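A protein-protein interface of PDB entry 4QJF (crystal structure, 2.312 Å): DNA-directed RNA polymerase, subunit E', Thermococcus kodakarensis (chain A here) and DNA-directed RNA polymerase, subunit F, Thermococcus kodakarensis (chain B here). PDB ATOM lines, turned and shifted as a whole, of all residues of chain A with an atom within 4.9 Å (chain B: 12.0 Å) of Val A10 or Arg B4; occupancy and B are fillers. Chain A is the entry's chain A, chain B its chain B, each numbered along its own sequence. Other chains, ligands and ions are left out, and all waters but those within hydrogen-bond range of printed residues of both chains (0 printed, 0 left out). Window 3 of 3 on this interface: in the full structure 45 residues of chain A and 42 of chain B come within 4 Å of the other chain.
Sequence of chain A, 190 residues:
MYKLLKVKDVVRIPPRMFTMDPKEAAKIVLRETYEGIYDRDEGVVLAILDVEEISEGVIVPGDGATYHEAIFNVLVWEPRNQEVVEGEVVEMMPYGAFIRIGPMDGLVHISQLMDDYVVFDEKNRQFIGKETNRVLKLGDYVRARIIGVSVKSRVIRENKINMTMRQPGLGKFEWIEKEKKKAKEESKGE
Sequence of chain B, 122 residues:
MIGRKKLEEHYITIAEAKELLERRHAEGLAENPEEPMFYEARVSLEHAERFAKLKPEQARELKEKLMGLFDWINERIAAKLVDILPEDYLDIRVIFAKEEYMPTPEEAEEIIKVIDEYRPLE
OD1 of Asp A9 lies within salt-bridge range of NH1 of Arg B4, 3.7 Å away. N of Arg B4 sits at hydrogen-bond distance from O of Lys A8. The backbone NH (N) of Lys A8 lies within hydrogen-bond range of the backbone carbonyl oxygen (O) of Lys B5, 3.3 Å away.
Among the printed residues, merely in contact across the chains: Val A7 with Ile B2 (3.3 Å), Asp A9 with Gly B3 (3.3 Å), Val A10 with Arg B4 (3.5 Å), Lys A8 with Leu B7 (3.6 Å), Val A7 with Gly B3 (3.8 Å), Val A7 with Lys B5 (3.8 Å), Val A7 with Leu B7 (3.9 Å) and Lys A8 with Gly B3 (3.9 Å).
Val A10 touches just one residue of chain B: Arg B4. Arg B4 touches three residues of chain A. No residue of chain B comes within 4 Å of Val A11. Printed residues of chain B within 4 Å of Val A7: Ile B2, Gly B3, Lys B5 and Leu B7. Of the printed residues of chain A, Lys B5 touches Val A7 (3.8 Å) and Lys A8 (3.3 Å). Of the printed residues of chain A, Ile B2 touches Val A7 (3.3 Å).
Of the 8 printed residues of chain A, 4 touch a printed residue of chain B. Among the printed residues, 11 pairs touch across the chains. Among the printed residues, Asp or Glu carboxylates within 4 Å of a Lys or Arg side-chain nitrogen of the other chain: Asp A9 with Arg B4 (3.7 Å).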
ATOM      1  N   VAL A   7       9.996 -28.766  33.393  1.00  0.00           N
ATOM      2  CA  VAL A   7      10.193 -27.908  32.237  1.00  0.00           C
ATOM      3  C   VAL A   7      11.329 -28.434  31.344  1.00  0.00           C
ATOM      4  O   VAL A   7      12.326 -28.983  31.832  1.00  0.00           O
ATOM      5  CB  VAL A   7      10.487 -26.452  32.701  1.00  0.00           C
ATOM      6  CG1 VAL A   7      11.001 -25.573  31.566  1.00  0.00           C
ATOM      7  CG2 VAL A   7       9.237 -25.842  33.338  1.00  0.00           C
ATOM      8  N   LYS A   8      11.151 -28.286  30.033  1.00  0.00           N
ATOM      9  CA  LYS A   8      12.201 -28.586  29.072  1.00  0.00           C
ATOM     10  C   LYS A   8      12.680 -27.273  28.483  1.00  0.00           C
ATOM     11  O   LYS A   8      11.875 -26.379  28.227  1.00  0.00           O
ATOM     12  CB  LYS A   8      11.698 -29.532  27.978  1.00  0.00           C
ATOM     13  CG  LYS A   8      10.786 -30.632  28.493  1.00  0.00           C
ATOM     14  CD  LYS A   8      10.470 -31.657  27.411  1.00  0.00           C
ATOM     15  CE  LYS A   8       9.465 -32.706  27.886  1.00  0.00           C
ATOM     16  NZ  LYS A   8       9.223 -33.735  26.834  1.00  0.00           N
ATOM     17  N   ASP A   9      13.991 -27.141  28.301  1.00  0.00           N
ATOM     18  CA  ASP A   9      14.582 -25.874  27.870  1.00  0.00           C
ATOM     19  C   ASP A   9      15.898 -26.095  27.121  1.00  0.00           C
ATOM     20  O   ASP A   9      16.455 -27.197  27.129  1.00  0.00           O
ATOM     21  CB  ASP A   9      14.820 -24.954  29.081  1.00  0.00           C
ATOM     22  CG  ASP A   9      14.854 -23.475  28.709  1.00  0.00           C
ATOM     23  OD1 ASP A   9      14.753 -23.134  27.516  1.00  0.00           O
ATOM     24  OD2 ASP A   9      14.989 -22.640  29.618  1.00  0.00           O
ATOM     25  N   VAL A  10      16.392 -25.037  26.484  1.00  0.00           N
ATOM     26  CA  VAL A  10      17.696 -25.071  25.849  1.00  0.00           C
ATOM     27  C   VAL A  10      18.680 -24.211  26.623  1.00  0.00           C
ATOM     28  O   VAL A  10      18.463 -23.016  26.773  1.00  0.00           O
ATOM     29  CB  VAL A  10      17.621 -24.588  24.388  1.00  0.00           C
ATOM     30  CG1 VAL A  10      19.029 -24.333  23.816  1.00  0.00           C
ATOM     31  CG2 VAL A  10      16.852 -25.605  23.544  1.00  0.00           C
ATOM     32  N   VAL A  11      19.757 -24.822  27.113  1.00  0.00           N
ATOM     33  CA  VAL A  11      20.780 -24.097  27.875  1.00  0.00           C
ATOM     34  C   VAL A  11      22.119 -23.964  27.145  1.00  0.00           C
ATOM     35  O   VAL A  11      22.579 -24.894  26.467  1.00  0.00           O
ATOM     36  CB  VAL A  11      21.080 -24.759  29.249  1.00  0.00           C
ATOM     37  CG1 VAL A  11      20.572 -23.892  30.391  1.00  0.00           C
ATOM     38  CG2 VAL A  11      20.515 -26.173  29.319  1.00  0.00           C
ATOM     39  N   ARG A  12      22.737 -22.797  27.316  1.00  0.00           N
ATOM     40  CA  ARG A  12      24.077 -22.537  26.827  1.00  0.00           C
ATOM     41  C   ARG A  12      25.052 -22.703  27.975  1.00  0.00           C
ATOM     42  O   ARG A  12      25.050 -21.907  28.914  1.00  0.00           O
ATOM     43  CB  ARG A  12      24.180 -21.123  26.231  1.00  0.00           C
ATOM     44  CG  ARG A  12      25.584 -20.709  25.807  1.00  0.00           C
ATOM     45  CD  ARG A  12      25.604 -19.328  25.122  1.00  0.00           C
ATOM     46  NE  ARG A  12      26.914 -19.030  24.535  1.00  0.00           N
ATOM     47  CZ  ARG A  12      27.976 -18.623  25.228  1.00  0.00           C
ATOM     48  NH1 ARG A  12      27.879 -18.445  26.540  1.00  0.00           N
ATOM     49  NH2 ARG A  12      29.135 -18.396  24.613  1.00  0.00           N
ATOM     50  N   HIS A  68      22.980 -27.608  25.042  1.00  0.00           N
ATOM     51  CA  HIS A  68      22.208 -28.806  25.361  1.00  0.00           C
ATOM     52  C   HIS A  68      20.717 -28.504  25.485  1.00  0.00           C
ATOM     53  O   HIS A  68      20.303 -27.357  25.655  1.00  0.00           O
ATOM     54  CB  HIS A  68      22.662 -29.440  26.679  1.00  0.00           C
ATOM     55  CG  HIS A  68      24.133 -29.708  26.783  1.00  0.00           C
ATOM     56  ND1 HIS A  68      24.655 -30.986  26.759  1.00  0.00           N
ATOM     57  CD2 HIS A  68      25.182 -28.876  26.979  1.00  0.00           C
ATOM     58  CE1 HIS A  68      25.966 -30.924  26.914  1.00  0.00           C
ATOM     59  NE2 HIS A  68      26.315 -29.658  27.048  1.00  0.00           N
ATOM     60  N   GLU A  69      19.908 -29.552  25.412  1.00  0.00           N
ATOM     61  CA  GLU A  69      18.516 -29.449  25.812  1.00  0.00           C
ATOM     62  C   GLU A  69      18.383 -30.151  27.150  1.00  0.00           C
ATOM     63  O   GLU A  69      18.954 -31.227  27.345  1.00  0.00           O
ATOM     64  CB  GLU A  69      17.590 -30.055  24.770  1.00  0.00           C
ATOM     65  CG  GLU A  69      16.126 -29.770  25.029  1.00  0.00           C
ATOM     66  CD  GLU A  69      15.323 -29.698  23.749  1.00  0.00           C
ATOM     67  OE1 GLU A  69      15.910 -29.350  22.699  1.00  0.00           O
ATOM     68  OE2 GLU A  69      14.110 -29.993  23.793  1.00  0.00           O
ATOM     69  N   MET B   1       6.389 -17.687  30.585  1.00  0.00           N
ATOM     70  CA  MET B   1       6.707 -19.116  30.619  1.00  0.00           C
ATOM     71  C   MET B   1       8.160 -19.390  30.995  1.00  0.00           C
ATOM     72  O   MET B   1       9.080 -18.724  30.524  1.00  0.00           O
ATOM     73  CB  MET B   1       6.408 -19.780  29.267  1.00  0.00           C
ATOM     74  CG  MET B   1       4.932 -19.833  28.900  1.00  0.00           C
ATOM     75  SD  MET B   1       3.887 -20.594  30.166  1.00  0.00           S
ATOM     76  CE  MET B   1       4.495 -22.281  30.156  1.00  0.00           C
ATOM     77  N   ILE B   2       8.345 -20.383  31.855  1.00  0.00           N
ATOM     78  CA  ILE B   2       9.664 -20.904  32.162  1.00  0.00           C
ATOM     79  C   ILE B   2      10.044 -21.902  31.079  1.00  0.00           C
ATOM     80  O   ILE B   2       9.324 -22.873  30.855  1.00  0.00           O
ATOM     81  CB  ILE B   2       9.699 -21.596  33.544  1.00  0.00           C
ATOM     82  CG1 ILE B   2       8.897 -20.793  34.567  1.00  0.00           C
ATOM     83  CG2 ILE B   2      11.132 -21.781  34.021  1.00  0.00           C
ATOM     84  CD1 ILE B   2       9.437 -19.407  34.779  1.00  0.00           C
ATOM     85  N   GLY B   3      11.157 -21.651  30.394  1.00  0.00           N
ATOM     86  CA  GLY B   3      11.651 -22.564  29.369  1.00  0.00           C
ATOM     87  C   GLY B   3      10.803 -22.618  28.114  1.00  0.00           C
ATOM     88  O   GLY B   3       9.947 -21.764  27.901  1.00  0.00           O
ATOM     89  N   ARG B   4      11.043 -23.634  27.288  1.00  0.00           N
ATOM     90  CA  ARG B   4      10.346 -23.805  26.013  1.00  0.00           C
ATOM     91  C   ARG B   4       8.907 -24.310  26.166  1.00  0.00           C
ATOM     92  O   ARG B   4       7.973 -23.707  25.640  1.00  0.00           O
ATOM     93  CB  ARG B   4      11.124 -24.767  25.118  1.00  0.00           C
ATOM     94  CG  ARG B   4      12.507 -24.287  24.738  1.00  0.00           C
ATOM     95  CD  ARG B   4      12.450 -23.308  23.583  1.00  0.00           C
ATOM     96  NE  ARG B   4      13.765 -23.118  22.978  1.00  0.00           N
ATOM     97  CZ  ARG B   4      14.627 -22.177  23.347  1.00  0.00           C
ATOM     98  NH1 ARG B   4      14.313 -21.333  24.323  1.00  0.00           N
ATOM     99  NH2 ARG B   4      15.803 -22.076  22.739  1.00  0.00           N
ATOM    100  N   LYS B   5       8.729 -25.427  26.862  1.00  0.00           N
ATOM    101  CA  LYS B   5       7.385 -25.903  27.167  1.00  0.00           C
ATOM    102  C   LYS B   5       7.292 -26.513  28.562  1.00  0.00           C
ATOM    103  O   LYS B   5       8.246 -27.109  29.074  1.00  0.00           O
ATOM    104  CB  LYS B   5       6.919 -26.925  26.129  1.00  0.00           C
ATOM    105  CG  LYS B   5       7.708 -28.220  26.145  1.00  0.00           C
ATOM    106  CD  LYS B   5       6.819 -29.448  26.375  1.00  0.00           C
ATOM    107  CE  LYS B   5       6.159 -29.921  25.083  1.00  0.00           C
ATOM    108  NZ  LYS B   5       5.937 -31.395  25.069  1.00  0.00           N
ATOM    109  N   LYS B   6       6.131 -26.336  29.177  1.00  0.00           N
ATOM    110  CA  LYS B   6       5.818 -27.001  30.430  1.00  0.00           C
ATOM    111  C   LYS B   6       5.338 -28.407  30.111  1.00  0.00           C
ATOM    112  O   LYS B   6       4.443 -28.591  29.294  1.00  0.00           O
ATOM    113  CB  LYS B   6       4.755 -26.223  31.222  1.00  0.00           C
ATOM    114  CG  LYS B   6       4.319 -26.914  32.511  1.00  0.00           C
ATOM    115  CD  LYS B   6       3.753 -25.926  33.522  1.00  0.00           C
ATOM    116  CE  LYS B   6       2.496 -25.260  33.002  1.00  0.00           C
ATOM    117  NZ  LYS B   6       1.952 -24.282  33.973  1.00  0.00           N
ATOM    118  N   LEU B   7       5.936 -29.409  30.735  1.00  0.00           N
ATOM    119  CA  LEU B   7       5.469 -30.753  30.486  1.00  0.00           C
ATOM    120  C   LEU B   7       4.615 -31.312  31.638  1.00  0.00           C
ATOM    121  O   LEU B   7       3.799 -32.216  31.423  1.00  0.00           O
ATOM    122  CB  LEU B   7       6.654 -31.668  30.199  1.00  0.00           C
ATOM    123  CG  LEU B   7       7.390 -32.282  31.377  1.00  0.00           C
ATOM    124  CD1 LEU B   7       7.264 -33.796  31.295  1.00  0.00           C
ATOM    125  CD2 LEU B   7       8.845 -31.860  31.344  1.00  0.00           C
ATOM    126  N   GLU B   8       4.776 -30.768  32.845  1.00  0.00           N
ATOM    127  CA  GLU B   8       4.123 -31.338  34.026  1.00  0.00           C
ATOM    128  C   GLU B   8       4.108 -30.368  35.206  1.00  0.00           C
ATOM    129  O   GLU B   8       5.086 -29.661  35.456  1.00  0.00           O
ATOM    130  CB  GLU B   8       4.820 -32.647  34.430  1.00  0.00           C
ATOM    131  CG  GLU B   8       4.203 -33.367  35.620  1.00  0.00           C
ATOM    132  CD  GLU B   8       4.779 -34.765  35.825  1.00  0.00           C
ATOM    133  OE1 GLU B   8       5.441 -35.277  34.895  1.00  0.00           O
ATOM    134  OE2 GLU B   8       4.574 -35.352  36.913  1.00  0.00           O
